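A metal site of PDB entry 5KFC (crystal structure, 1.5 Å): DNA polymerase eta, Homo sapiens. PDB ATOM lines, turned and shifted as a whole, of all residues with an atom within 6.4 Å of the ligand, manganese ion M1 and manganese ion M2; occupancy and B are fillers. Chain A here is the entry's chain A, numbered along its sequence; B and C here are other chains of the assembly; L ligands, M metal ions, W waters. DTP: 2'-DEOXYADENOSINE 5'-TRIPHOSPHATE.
Merely in contact with manganese ion M2: Lys 234 (3.7 Å). The nearest printed residue that does not touch manganese ion M2 is Asp 18 (4.4 Å).
Water W8 bridges NZ of Lys 227 (2.9 Å) and O2A of the ligand (3.5 Å). Water W7 lies within hydrogen-bond range of O2 of DT 8 of chain B (2.7 Å) and an oxygen (O4') of the ligand (3.4 Å).
N1 of the ligand lies close to N1 of DA 5 of chain C. Asp 18 touches the ligand (CA to O2G, 3.4 Å). O of Ile 51 touches C2' of the ligand (3.4 Å). Ala 52 touches the ligand (CB to O3', 3.5 Å). CG2 of Ile 117 touches O4' of the ligand, at 3.7 Å. Hydrophobic or aromatic side chains that line the ligand: Phe 20, Phe 21, Ile 51, Ala 52, Tyr 55 and Ile 117. Within 4 Å of the ligand: Asp 16, Met 17, Asp 18, Cys 19, Phe 20, Phe 21, Ile 51, Ala 52, Tyr 55, Arg 58, Arg 64, Ile 117, Asp 118, Lys 234, DT 8 of chain B, DT 4 of chain C and DA 5 of chain C. Along chain A the residues within 4 Å of the ligand span positions 16 to 234.
Manganese ion M1 is bound by the side-chain carboxylate (OD2) of Asp 16, the side-chain carboxylate (OE2) of Glu 119, water W8, an oxygen (O1A) of the ligand, the side-chain carboxylate (OD1) of Asp 118 and O3' of DT 8 of chain B.
N6 of the ligand is in hydrogen-bond range of N3 of DT 8 of chain B (3.4 Å). OH of Tyr 55 sits at hydrogen-bond distance from O2G of the ligand, 2.6 Å away. O4 of DT 4 of chain C is in hydrogen-bond range of a nitrogen (N6) of the ligand (3.0 Å). The backbone NH (N) of Cys 19 sits at hydrogen-bond distance from an oxygen (O2G) of the ligand (2.8 Å). NH1 of Arg 58 lies within salt-bridge range of O3G of the ligand (3.1 Å). N of Phe 20 is in hydrogen-bond range of O2B of the ligand, at 3.5 Å. O2B of the ligand lies within salt-bridge range of NH2 of Arg 64 (3.1 Å). The backbone NH (N) of Phe 21 sits at hydrogen-bond distance from an oxygen (O3') of the ligand (3.1 Å). The side-chain amino group of Lys 234 lies within salt-bridge range of an oxygen (O2G) of the ligand (3.3 Å).
Merely in contact with manganese ion M1: Ser 116 (3.8 Å). Five residues have an atom within 4 Å of manganese ion M1: Asp 16, Ser 116, Asp 118, Glu 119 and DT 8 of chain B.
Manganese ion M2 is bound by OD1 of Asp 16 (2.2 Å), O of Met 17 (2.2 Å), OD2 of Asp 118 (2.2 Å), O1G of the ligand (2.2 Å), O1B of the ligand (2.3 Å) and O1A of the ligand (2.4 Å).
The backbone carbonyl oxygen of Asp 16 lies within hydrogen-bond range of the backbone NH of Ser 216, 2.9 Å away. OG of Ser 116 sits at hydrogen-bond distance from N of Glu 119 (3.2 Å). The side-chain amino group (NZ) of Lys 227 is in salt-bridge range of the side-chain carboxylate (OE1) of Glu 119. The side-chain amino group of Lys 234 sits close to the backbone carbonyl oxygen of Met 17 (3.2 Å). The side-chain hydroxyl of Ser 116 sits at hydrogen-bond distance from the backbone NH of Asp 118, 3.0 Å away. O2 of DT 4 of chain C lies within hydrogen-bond range of the side-chain amide nitrogen (NE2) of Gln 41 (2.7 Å). The guanidinium group (NE) of Arg 58 lies within hydrogen-bond range of the backbone carbonyl oxygen (O) of Val 53 (3.0 Å). NE of Arg 64 sits at hydrogen-bond distance from O of Ile 51 (2.8 Å).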
ATOM      1  N   ASP A  16     -31.011   6.595 -22.987  1.00  0.00           N
ATOM      2  CA  ASP A  16     -30.287   6.683 -21.731  1.00  0.00           C
ATOM      3  C   ASP A  16     -31.068   7.501 -20.722  1.00  0.00           C
ATOM      4  O   ASP A  16     -31.453   8.635 -20.998  1.00  0.00           O
ATOM      5  CB  ASP A  16     -28.903   7.294 -21.930  1.00  0.00           C
ATOM      6  CG  ASP A  16     -28.161   7.453 -20.637  1.00  0.00           C
ATOM      7  OD1 ASP A  16     -28.351   8.486 -19.976  1.00  0.00           O
ATOM      8  OD2 ASP A  16     -27.389   6.537 -20.275  1.00  0.00           O
ATOM      9  N   MET A  17     -31.301   6.937 -19.546  1.00  0.00           N
ATOM     10  CA  MET A  17     -32.130   7.613 -18.557  1.00  0.00           C
ATOM     11  C   MET A  17     -31.461   8.878 -18.007  1.00  0.00           C
ATOM     12  O   MET A  17     -30.266   8.900 -17.809  1.00  0.00           O
ATOM     13  CB  MET A  17     -32.469   6.661 -17.403  1.00  0.00           C
ATOM     14  CG  MET A  17     -33.084   5.346 -17.862  1.00  0.00           C
ATOM     15  SD  MET A  17     -34.554   5.507 -18.895  1.00  0.00           S
ATOM     16  CE  MET A  17     -35.688   6.213 -17.761  1.00  0.00           C
ATOM     17  N   ASP A  18     -32.250   9.929 -17.771  1.00  0.00           N
ATOM     18  CA  ASP A  18     -31.682  11.142 -17.170  1.00  0.00           C
ATOM     19  C   ASP A  18     -31.458  10.965 -15.671  1.00  0.00           C
ATOM     20  O   ASP A  18     -32.376  10.509 -14.951  1.00  0.00           O
ATOM     21  CB  ASP A  18     -32.623  12.332 -17.340  1.00  0.00           C
ATOM     22  CG  ASP A  18     -32.887  12.672 -18.797  1.00  0.00           C
ATOM     23  OD1 ASP A  18     -32.049  12.395 -19.663  1.00  0.00           O
ATOM     24  OD2 ASP A  18     -33.967  13.224 -19.046  1.00  0.00           O
ATOM     25  N   CYS A  19     -30.246  11.301 -15.230  1.00  0.00           N
ATOM     26  CA  CYS A  19     -29.816  11.231 -13.817  1.00  0.00           C
ATOM     27  C   CYS A  19     -30.539  10.078 -13.109  1.00  0.00           C
ATOM     28  O   CYS A  19     -31.295  10.287 -12.168  1.00  0.00           O
ATOM     29  CB  CYS A  19     -30.016  12.568 -13.070  1.00  0.00           C
ATOM     30  SG  CYS A  19     -31.622  13.391 -13.144  1.00  0.00           S
ATOM     31  N   PHE A  20     -30.286   8.862 -13.581  1.00  0.00           N
ATOM     32  CA  PHE A  20     -31.197   7.754 -13.329  1.00  0.00           C
ATOM     33  C   PHE A  20     -31.469   7.465 -11.850  1.00  0.00           C
ATOM     34  O   PHE A  20     -32.631   7.446 -11.459  1.00  0.00           O
ATOM     35  CB  PHE A  20     -30.676   6.465 -14.010  1.00  0.00           C
ATOM     36  CG  PHE A  20     -31.610   5.281 -13.886  1.00  0.00           C
ATOM     37  CD1 PHE A  20     -32.975   5.418 -14.152  1.00  0.00           C
ATOM     38  CD2 PHE A  20     -31.131   4.035 -13.512  1.00  0.00           C
ATOM     39  CE1 PHE A  20     -33.832   4.313 -14.060  1.00  0.00           C
ATOM     40  CE2 PHE A  20     -31.999   2.943 -13.415  1.00  0.00           C
ATOM     41  CZ  PHE A  20     -33.344   3.098 -13.692  1.00  0.00           C
ATOM     42  N   PHE A  21     -30.440   7.262 -11.034  1.00  0.00           N
ATOM     43  CA  PHE A  21     -30.721   6.892  -9.649  1.00  0.00           C
ATOM     44  C   PHE A  21     -31.477   8.022  -8.927  1.00  0.00           C
ATOM     45  O   PHE A  21     -32.273   7.766  -8.031  1.00  0.00           O
ATOM     46  CB  PHE A  21     -29.456   6.551  -8.853  1.00  0.00           C
ATOM     47  CG  PHE A  21     -28.772   5.273  -9.237  1.00  0.00           C
ATOM     48  CD1 PHE A  21     -29.113   4.570 -10.404  1.00  0.00           C
ATOM     49  CD2 PHE A  21     -27.764   4.766  -8.430  1.00  0.00           C
ATOM     50  CE1 PHE A  21     -28.452   3.387 -10.733  1.00  0.00           C
ATOM     51  CE2 PHE A  21     -27.109   3.584  -8.750  1.00  0.00           C
ATOM     52  CZ  PHE A  21     -27.442   2.898  -9.912  1.00  0.00           C
ATOM     53  N   VAL A  22     -31.207   9.271  -9.314  1.00  0.00           N
ATOM     54  CA  VAL A  22     -31.937  10.394  -8.723  1.00  0.00           C
ATOM     55  C   VAL A  22     -33.414  10.313  -9.082  1.00  0.00           C
ATOM     56  O   VAL A  22     -34.284  10.457  -8.213  1.00  0.00           O
ATOM     57  CB  VAL A  22     -31.335  11.748  -9.176  1.00  0.00           C
ATOM     58  CG1 VAL A  22     -32.308  12.896  -8.894  1.00  0.00           C
ATOM     59  CG2 VAL A  22     -29.999  11.990  -8.477  1.00  0.00           C
ATOM     60  N   GLN A  41     -23.691   7.062  -1.500  1.00  0.00           N
ATOM     61  CA  GLN A  41     -23.555   5.775  -0.806  1.00  0.00           C
ATOM     62  C   GLN A  41     -22.565   5.920   0.335  1.00  0.00           C
ATOM     63  O   GLN A  41     -21.499   6.542   0.210  1.00  0.00           O
ATOM     64  CB  GLN A  41     -23.181   4.630  -1.765  1.00  0.00           C
ATOM     65  CG  GLN A  41     -21.981   4.811  -2.643  1.00  0.00           C
ATOM     66  CD  GLN A  41     -21.859   3.701  -3.704  1.00  0.00           C
ATOM     67  OE1 GLN A  41     -22.715   2.804  -3.827  1.00  0.00           O
ATOM     68  NE2 GLN A  41     -20.785   3.764  -4.461  1.00  0.00           N
ATOM     69  N   ILE A  51     -23.041   9.401  -6.342  1.00  0.00           N
ATOM     70  CA  ILE A  51     -23.002   8.600  -7.572  1.00  0.00           C
ATOM     71  C   ILE A  51     -24.028   9.039  -8.616  1.00  0.00           C
ATOM     72  O   ILE A  51     -23.986   8.565  -9.738  1.00  0.00           O
ATOM     73  CB  ILE A  51     -23.195   7.090  -7.284  1.00  0.00           C
ATOM     74  CG1 ILE A  51     -24.535   6.799  -6.596  1.00  0.00           C
ATOM     75  CG2 ILE A  51     -22.007   6.553  -6.479  1.00  0.00           C
ATOM     76  CD1 ILE A  51     -24.851   5.303  -6.488  1.00  0.00           C
ATOM     77  N   ALA A  52     -24.914   9.976  -8.276  1.00  0.00           N
ATOM     78  CA  ALA A  52     -25.860  10.520  -9.262  1.00  0.00           C
ATOM     79  C   ALA A  52     -26.315  11.905  -8.808  1.00  0.00           C
ATOM     80  O   ALA A  52     -26.452  12.135  -7.602  1.00  0.00           O
ATOM     81  CB  ALA A  52     -27.082   9.595  -9.448  1.00  0.00           C
ATOM     82  N   VAL A  53     -26.575  12.803  -9.761  1.00  0.00           N
ATOM     83  CA  VAL A  53     -26.803  14.232  -9.475  1.00  0.00           C
ATOM     84  C   VAL A  53     -27.919  14.790 -10.339  1.00  0.00           C
ATOM     85  O   VAL A  53     -27.862  14.646 -11.570  1.00  0.00           O
ATOM     86  CB  VAL A  53     -25.523  15.073  -9.732  1.00  0.00           C
ATOM     87  CG1 VAL A  53     -25.718  16.516  -9.272  1.00  0.00           C
ATOM     88  CG2 VAL A  53     -24.326  14.481  -9.020  1.00  0.00           C
ATOM     89  N   TYR A  55     -30.147  17.608 -12.351  1.00  0.00           N
ATOM     90  CA  TYR A  55     -29.664  18.697 -13.187  1.00  0.00           C
ATOM     91  C   TYR A  55     -29.694  20.018 -12.437  1.00  0.00           C
ATOM     92  O   TYR A  55     -28.821  20.871 -12.650  1.00  0.00           O
ATOM     93  CB  TYR A  55     -30.461  18.736 -14.500  1.00  0.00           C
ATOM     94  CG  TYR A  55     -29.937  17.681 -15.448  1.00  0.00           C
ATOM     95  CD1 TYR A  55     -30.335  16.353 -15.331  1.00  0.00           C
ATOM     96  CD2 TYR A  55     -28.989  17.996 -16.419  1.00  0.00           C
ATOM     97  CE1 TYR A  55     -29.822  15.362 -16.175  1.00  0.00           C
ATOM     98  CE2 TYR A  55     -28.489  17.037 -17.273  1.00  0.00           C
ATOM     99  CZ  TYR A  55     -28.890  15.717 -17.146  1.00  0.00           C
ATOM    100  OH  TYR A  55     -28.382  14.749 -17.982  1.00  0.00           O
ATOM    101  N   ARG A  58     -26.476  20.020 -10.606  1.00  0.00           N
ATOM    102  CA  ARG A  58     -25.333  20.193 -11.489  1.00  0.00           C
ATOM    103  C   ARG A  58     -25.061  21.675 -11.755  1.00  0.00           C
ATOM    104  O   ARG A  58     -23.910  22.049 -11.961  1.00  0.00           O
ATOM    105  CB  ARG A  58     -25.532  19.468 -12.824  1.00  0.00           C
ATOM    106  CG  ARG A  58     -25.676  17.973 -12.663  1.00  0.00           C
ATOM    107  CD  ARG A  58     -25.824  17.260 -13.997  1.00  0.00           C
ATOM    108  NE  ARG A  58     -26.296  15.894 -13.760  1.00  0.00           N
ATOM    109  CZ  ARG A  58     -26.337  14.931 -14.671  1.00  0.00           C
ATOM    110  NH1 ARG A  58     -25.928  15.170 -15.908  1.00  0.00           N
ATOM    111  NH2 ARG A  58     -26.794  13.717 -14.325  1.00  0.00           N
ATOM    112  N   ARG A  64     -20.733  13.662  -9.854  1.00  0.00           N
ATOM    113  CA  ARG A  64     -20.403  12.316  -9.427  1.00  0.00           C
ATOM    114  C   ARG A  64     -18.969  12.256  -8.872  1.00  0.00           C
ATOM    115  O   ARG A  64     -18.113  13.037  -9.272  1.00  0.00           O
ATOM    116  CB  ARG A  64     -20.574  11.355 -10.610  1.00  0.00           C
ATOM    117  CG  ARG A  64     -20.084   9.942 -10.412  1.00  0.00           C
ATOM    118  CD  ARG A  64     -20.484   9.092 -11.608  1.00  0.00           C
ATOM    119  NE  ARG A  64     -21.938   9.035 -11.662  1.00  0.00           N
ATOM    120  CZ  ARG A  64     -22.674   9.208 -12.757  1.00  0.00           C
ATOM    121  NH1 ARG A  64     -22.112   9.426 -13.953  1.00  0.00           N
ATOM    122  NH2 ARG A  64     -23.991   9.150 -12.658  1.00  0.00           N
ATOM    123  N   LEU A  92     -27.796  -2.391  -4.533  1.00  0.00           N
ATOM    124  CA  LEU A  92     -28.332  -1.601  -5.642  1.00  0.00           C
ATOM    125  C   LEU A  92     -29.626  -2.183  -6.240  1.00  0.00           C
ATOM    126  O   LEU A  92     -30.002  -1.829  -7.355  1.00  0.00           O
ATOM    127  CB  LEU A  92     -27.286  -1.468  -6.747  1.00  0.00           C
ATOM    128  CG  LEU A  92     -25.930  -0.919  -6.315  1.00  0.00           C
ATOM    129  CD1 LEU A  92     -24.949  -1.000  -7.478  1.00  0.00           C
ATOM    130  CD2 LEU A  92     -26.081   0.536  -5.847  1.00  0.00           C
ATOM    131  N   SER A 116     -25.966  -0.719 -20.100  1.00  0.00           N
ATOM    132  CA  SER A 116     -25.697  -0.353 -18.716  1.00  0.00           C
ATOM    133  C   SER A 116     -26.969  -0.483 -17.906  1.00  0.00           C
ATOM    134  O   SER A 116     -28.022  -0.815 -18.440  1.00  0.00           O
ATOM    135  CB  SER A 116     -25.166   1.087 -18.598  1.00  0.00           C
ATOM    136  OG  SER A 116     -26.213   2.033 -18.630  1.00  0.00           O
ATOM    137  N   ILE A 117     -26.891  -0.163 -16.627  1.00  0.00           N
ATOM    138  CA  ILE A 117     -28.080  -0.197 -15.807  1.00  0.00           C
ATOM    139  C   ILE A 117     -29.133   0.801 -16.307  1.00  0.00           C
ATOM    140  O   ILE A 117     -30.314   0.642 -16.028  1.00  0.00           O
ATOM    141  CB  ILE A 117     -27.737   0.084 -14.316  1.00  0.00           C
ATOM    142  CG1 ILE A 117     -28.867  -0.407 -13.403  1.00  0.00           C
ATOM    143  CG2 ILE A 117     -27.412   1.564 -14.078  1.00  0.00           C
ATOM    144  CD1 ILE A 117     -28.444  -0.477 -11.944  1.00  0.00           C
ATOM    145  N   ASP A 118     -28.743   1.835 -17.050  1.00  0.00           N
ATOM    146  CA  ASP A 118     -29.747   2.823 -17.400  1.00  0.00           C
ATOM    147  C   ASP A 118     -29.780   3.145 -18.896  1.00  0.00           C
ATOM    148  O   ASP A 118     -30.339   4.186 -19.301  1.00  0.00           O
ATOM    149  CB  ASP A 118     -29.538   4.117 -16.595  1.00  0.00           C
ATOM    150  CG  ASP A 118     -28.560   5.077 -17.244  1.00  0.00           C
ATOM    151  OD1 ASP A 118     -27.549   4.651 -17.852  1.00  0.00           O
ATOM    152  OD2 ASP A 118     -28.879   6.300 -17.235  1.00  0.00           O
ATOM    153  N   GLU A 119     -29.230   2.269 -19.727  1.00  0.00           N
ATOM    154  CA  GLU A 119     -29.316   2.539 -21.162  1.00  0.00           C
ATOM    155  C   GLU A 119     -29.287   1.294 -22.014  1.00  0.00           C
ATOM    156  O   GLU A 119     -28.746   0.252 -21.623  1.00  0.00           O
ATOM    157  CB  GLU A 119     -28.199   3.467 -21.594  1.00  0.00           C
ATOM    158  CG  GLU A 119     -26.873   2.813 -21.733  1.00  0.00           C
ATOM    159  CD  GLU A 119     -25.754   3.799 -21.527  1.00  0.00           C
ATOM    160  OE1 GLU A 119     -25.160   4.246 -22.516  1.00  0.00           O
ATOM    161  OE2 GLU A 119     -25.484   4.137 -20.355  1.00  0.00           O
ATOM    162  N   SER A 216     -33.150  10.614 -22.342  1.00  0.00           N
ATOM    163  CA  SER A 216     -32.715  11.205 -23.592  1.00  0.00           C
ATOM    164  C   SER A 216     -32.434  10.097 -24.583  1.00  0.00           C
ATOM    165  O   SER A 216     -32.383   8.922 -24.220  1.00  0.00           O
ATOM    166  CB  SER A 216     -31.490  12.073 -23.366  1.00  0.00           C
ATOM    167  OG  SER A 216     -31.793  13.123 -22.452  1.00  0.00           O
ATOM    168  N   LYS A 227     -24.894   6.910 -29.431  1.00  0.00           N
ATOM    169  CA  LYS A 227     -24.448   7.259 -28.090  1.00  0.00           C
ATOM    170  C   LYS A 227     -24.000   8.722 -28.009  1.00  0.00           C
ATOM    171  O   LYS A 227     -24.361   9.456 -27.083  1.00  0.00           O
ATOM    172  CB  LYS A 227     -23.299   6.331 -27.656  1.00  0.00           C
ATOM    173  CG  LYS A 227     -22.739   6.651 -26.266  1.00  0.00           C
ATOM    174  CD  LYS A 227     -23.823   6.644 -25.191  1.00  0.00           C
ATOM    175  CE  LYS A 227     -23.226   6.860 -23.808  1.00  0.00           C
ATOM    176  NZ  LYS A 227     -24.217   6.793 -22.700  1.00  0.00           N
ATOM    177  N   LYS A 234     -29.159  16.448 -23.759  1.00  0.00           N
ATOM    178  CA  LYS A 234     -29.751  16.061 -22.444  1.00  0.00           C
ATOM    179  C   LYS A 234     -30.084  17.281 -21.569  1.00  0.00           C
ATOM    180  O   LYS A 234     -29.330  18.205 -21.623  1.00  0.00           O
ATOM    181  CB  LYS A 234     -28.737  15.219 -21.688  1.00  0.00           C
ATOM    182  CG  LYS A 234     -28.836  13.761 -21.944  1.00  0.00           C
ATOM    183  CD  LYS A 234     -28.121  12.827 -20.948  1.00  0.00           C
ATOM    184  CE  LYS A 234     -28.500  11.325 -21.226  1.00  0.00           C
ATOM    185  NZ  LYS A 234     -29.417  10.957 -20.118  1.00  0.00           N
ATOM    186  N   PRO A 235     -31.004  17.217 -20.608  1.00  0.00           N
ATOM    187  CA  PRO A 235     -31.887  16.067 -20.484  1.00  0.00           C
ATOM    188  C   PRO A 235     -33.231  16.152 -21.209  1.00  0.00           C
ATOM    189  O   PRO A 235     -33.563  17.144 -21.693  1.00  0.00           O
ATOM    190  CB  PRO A 235     -32.164  16.043 -18.977  1.00  0.00           C
ATOM    191  CG  PRO A 235     -32.297  17.448 -18.594  1.00  0.00           C
ATOM    192  CD  PRO A 235     -31.398  18.203 -19.461  1.00  0.00           C
ATOM    193  P    DT B   8     -20.279   4.625 -21.557  1.00  0.00           P
ATOM    194  OP1  DT B   8     -20.403   3.299 -22.185  1.00  0.00           O
ATOM    195  OP2  DT B   8     -20.682   5.836 -22.299  1.00  0.00           O
ATOM    196  O5'  DT B   8     -21.073   4.645 -20.189  1.00  0.00           O
ATOM    197  C5'  DT B   8     -21.997   3.685 -19.962  1.00  0.00           C
ATOM    198  C4'  DT B   8     -22.426   3.650 -18.507  1.00  0.00           C
ATOM    199  O4'  DT B   8     -21.407   3.148 -17.618  1.00  0.00           O
ATOM    200  C3'  DT B   8     -22.983   4.918 -17.853  1.00  0.00           C
ATOM    201  O3'  DT B   8     -24.365   4.755 -17.574  1.00  0.00           O
ATOM    202  C2'  DT B   8     -22.132   5.093 -16.578  1.00  0.00           C
ATOM    203  C1'  DT B   8     -21.609   3.688 -16.342  1.00  0.00           C
ATOM    204  N1   DT B   8     -20.324   3.654 -15.588  1.00  0.00           N
ATOM    205  C2   DT B   8     -20.252   2.941 -14.417  1.00  0.00           C
ATOM    206  O2   DT B   8     -21.189   2.345 -13.958  1.00  0.00           O
ATOM    207  N3   DT B   8     -19.021   2.978 -13.792  1.00  0.00           N
ATOM    208  C4   DT B   8     -17.883   3.628 -14.227  1.00  0.00           C
ATOM    209  O4   DT B   8     -16.833   3.607 -13.600  1.00  0.00           O
ATOM    210  C5   DT B   8     -18.034   4.352 -15.470  1.00  0.00           C
ATOM    211  C7   DT B   8     -16.867   5.099 -16.047  1.00  0.00           C
ATOM    212  C6   DT B   8     -19.228   4.327 -16.079  1.00  0.00           C
ATOM    213  P    DT C   3     -10.201   9.058  -2.773  1.00  0.00           P
ATOM    214  OP1  DT C   3      -8.931   8.422  -3.193  1.00  0.00           O
ATOM    215  OP2  DT C   3     -10.261  10.506  -2.486  1.00  0.00           O
ATOM    216  O5'  DT C   3     -11.311   8.702  -3.863  1.00  0.00           O
ATOM    217  C5'  DT C   3     -12.678   8.936  -3.582  1.00  0.00           C
ATOM    218  C4'  DT C   3     -13.564   8.152  -4.532  1.00  0.00           C
ATOM    219  O4'  DT C   3     -13.698   8.880  -5.775  1.00  0.00           O
ATOM    220  C3'  DT C   3     -13.008   6.765  -4.897  1.00  0.00           C
ATOM    221  O3'  DT C   3     -13.950   5.757  -4.557  1.00  0.00           O
ATOM    222  C2'  DT C   3     -12.739   6.848  -6.398  1.00  0.00           C
ATOM    223  C1'  DT C   3     -13.658   7.977  -6.851  1.00  0.00           C
ATOM    224  N1   DT C   3     -13.151   8.711  -8.038  1.00  0.00           N
ATOM    225  C2   DT C   3     -13.941   8.790  -9.159  1.00  0.00           C
ATOM    226  O2   DT C   3     -15.042   8.288  -9.238  1.00  0.00           O
ATOM    227  N3   DT C   3     -13.386   9.493 -10.195  1.00  0.00           N
ATOM    228  C4   DT C   3     -12.152  10.108 -10.232  1.00  0.00           C
ATOM    229  O4   DT C   3     -11.741  10.719 -11.212  1.00  0.00           O
ATOM    230  C5   DT C   3     -11.375   9.984  -9.019  1.00  0.00           C
ATOM    231  C7   DT C   3     -10.006  10.606  -8.929  1.00  0.00           C
ATOM    232  C6   DT C   3     -11.898   9.294  -7.996  1.00  0.00           C
ATOM    233  P    DT C   4     -13.524   4.597  -3.524  1.00  0.00           P
ATOM    234  OP1  DT C   4     -13.178   5.252  -2.239  1.00  0.00           O
ATOM    235  OP2  DT C   4     -12.518   3.776  -4.239  1.00  0.00           O
ATOM    236  O5'  DT C   4     -14.834   3.685  -3.363  1.00  0.00           O
ATOM    237  C5'  DT C   4     -15.857   3.989  -2.400  1.00  0.00           C
ATOM    238  C4'  DT C   4     -17.123   3.215  -2.734  1.00  0.00           C
ATOM    239  O4'  DT C   4     -17.606   3.673  -4.009  1.00  0.00           O
ATOM    240  C3'  DT C   4     -16.947   1.708  -2.870  1.00  0.00           C
ATOM    241  O3'  DT C   4     -18.142   1.072  -2.441  1.00  0.00           O
ATOM    242  C2'  DT C   4     -16.715   1.528  -4.381  1.00  0.00           C
ATOM    243  C1'  DT C   4     -17.663   2.585  -4.929  1.00  0.00           C
ATOM    244  N1   DT C   4     -17.339   3.143  -6.249  1.00  0.00           N
ATOM    245  C2   DT C   4     -18.386   3.444  -7.068  1.00  0.00           C
ATOM    246  O2   DT C   4     -19.544   3.192  -6.769  1.00  0.00           O
ATOM    247  N3   DT C   4     -18.045   4.002  -8.262  1.00  0.00           N
ATOM    248  C4   DT C   4     -16.787   4.332  -8.700  1.00  0.00           C
ATOM    249  O4   DT C   4     -16.595   4.844  -9.793  1.00  0.00           O
ATOM    250  C5   DT C   4     -15.718   4.013  -7.777  1.00  0.00           C
ATOM    251  C7   DT C   4     -14.288   4.317  -8.147  1.00  0.00           C
ATOM    252  C6   DT C   4     -16.044   3.463  -6.596  1.00  0.00           C
ATOM    253  P    DA C   5     -18.279  -0.522  -2.447  1.00  0.00           P
ATOM    254  OP1  DA C   5     -19.066  -0.861  -1.242  1.00  0.00           O
ATOM    255  OP2  DA C   5     -16.964  -1.127  -2.696  1.00  0.00           O
ATOM    256  O5'  DA C   5     -19.186  -0.808  -3.724  1.00  0.00           O
ATOM    257  C5'  DA C   5     -20.531  -0.365  -3.756  1.00  0.00           C
ATOM    258  C4'  DA C   5     -21.214  -0.839  -5.023  1.00  0.00           C
ATOM    259  O4'  DA C   5     -20.711  -0.091  -6.175  1.00  0.00           O
ATOM    260  C3'  DA C   5     -20.974  -2.317  -5.349  1.00  0.00           C
ATOM    261  O3'  DA C   5     -22.156  -2.848  -5.901  1.00  0.00           O
ATOM    262  C2'  DA C   5     -19.853  -2.248  -6.384  1.00  0.00           C
ATOM    263  C1'  DA C   5     -20.252  -1.006  -7.161  1.00  0.00           C
ATOM    264  N9   DA C   5     -19.170  -0.393  -7.888  1.00  0.00           N
ATOM    265  C8   DA C   5     -17.855  -0.327  -7.514  1.00  0.00           C
ATOM    266  N7   DA C   5     -17.098   0.328  -8.373  1.00  0.00           N
ATOM    267  C5   DA C   5     -17.984   0.724  -9.360  1.00  0.00           C
ATOM    268  C6   DA C   5     -17.809   1.451 -10.545  1.00  0.00           C
ATOM    269  N6   DA C   5     -16.629   1.925 -10.944  1.00  0.00           N
ATOM    270  N1   DA C   5     -18.897   1.677 -11.319  1.00  0.00           N
ATOM    271  C2   DA C   5     -20.084   1.202 -10.912  1.00  0.00           C
ATOM    272  N3   DA C   5     -20.372   0.504  -9.812  1.00  0.00           N
ATOM    273  C4   DA C   5     -19.260   0.299  -9.071  1.00  0.00           C
HETATM  274  PG  DTP L   1     -27.166  11.541 -17.124  1.00  0.00           P
HETATM  275  O1G DTP L   1     -27.144  10.300 -17.982  1.00  0.00           O
HETATM  276  O2G DTP L   1     -28.470  12.295 -17.207  1.00  0.00           O
HETATM  277  O3G DTP L   1     -25.980  12.473 -17.403  1.00  0.00           O
HETATM  278  PB  DTP L   1     -26.910   9.608 -15.025  1.00  0.00           P
HETATM  279  O1B DTP L   1     -28.064   8.796 -15.575  1.00  0.00           O
HETATM  280  O2B DTP L   1     -26.928   9.663 -13.513  1.00  0.00           O
HETATM  281  O3B DTP L   1     -27.001  11.118 -15.589  1.00  0.00           O
HETATM  282  PA  DTP L   1     -25.111   7.699 -16.234  1.00  0.00           P
HETATM  283  O1A DTP L   1     -25.939   7.381 -17.438  1.00  0.00           O
HETATM  284  O2A DTP L   1     -23.626   7.851 -16.547  1.00  0.00           O
HETATM  285  O3A DTP L   1     -25.504   9.072 -15.521  1.00  0.00           O
HETATM  286  O5' DTP L   1     -25.241   6.573 -15.131  1.00  0.00           O
HETATM  287  C5' DTP L   1     -26.476   5.982 -14.833  1.00  0.00           C
HETATM  288  C4' DTP L   1     -26.527   5.568 -13.361  1.00  0.00           C
HETATM  289  O4' DTP L   1     -25.504   4.623 -13.147  1.00  0.00           O
HETATM  290  C3' DTP L   1     -26.287   6.687 -12.467  1.00  0.00           C
HETATM  291  O3' DTP L   1     -27.511   7.380 -12.150  1.00  0.00           O
HETATM  292  C2' DTP L   1     -25.664   6.075 -11.284  1.00  0.00           C
HETATM  293  C1' DTP L   1     -24.914   4.920 -11.872  1.00  0.00           C
HETATM  294  N9  DTP L   1     -23.533   5.204 -12.065  1.00  0.00           N
HETATM  295  C8  DTP L   1     -22.951   5.821 -13.117  1.00  0.00           C
HETATM  296  N7  DTP L   1     -21.638   5.921 -12.933  1.00  0.00           N
HETATM  297  C5  DTP L   1     -21.330   5.332 -11.763  1.00  0.00           C
HETATM  298  C6  DTP L   1     -20.162   5.122 -11.043  1.00  0.00           C
HETATM  299  N6  DTP L   1     -18.909   5.567 -11.561  1.00  0.00           N
HETATM  300  N1  DTP L   1     -20.225   4.495  -9.863  1.00  0.00           N
HETATM  301  C2  DTP L   1     -21.384   4.052  -9.335  1.00  0.00           C
HETATM  302  N3  DTP L   1     -22.548   4.250 -10.015  1.00  0.00           N
HETATM  303  C4  DTP L   1     -22.533   4.877 -11.206  1.00  0.00           C
HETATM  304 MN    MN M   1     -25.966   5.766 -18.975  1.00  0.00          MN
HETATM  305 MN    MN M   2     -28.147   8.308 -17.804  1.00  0.00          MN
HETATM  306  O   HOH W   1     -25.132   9.899 -19.764  1.00  0.00           O
HETATM  307  O   HOH W   2     -23.588  12.379 -16.203  1.00  0.00           O
HETATM  308  O   HOH W   3     -24.103   2.195  -8.875  1.00  0.00           O
HETATM  309  O   HOH W   4     -19.391   7.193 -14.087  1.00  0.00           O
HETATM  310  O   HOH W   5     -25.883  11.878 -12.337  1.00  0.00           O
HETATM  311  O   HOH W   6     -24.807   3.341 -15.511  1.00  0.00           O
HETATM  312  O   HOH W   7     -23.580   1.805 -12.791  1.00  0.00           O
HETATM  313  O   HOH W   8     -24.483   7.144 -19.855  1.00  0.00           O
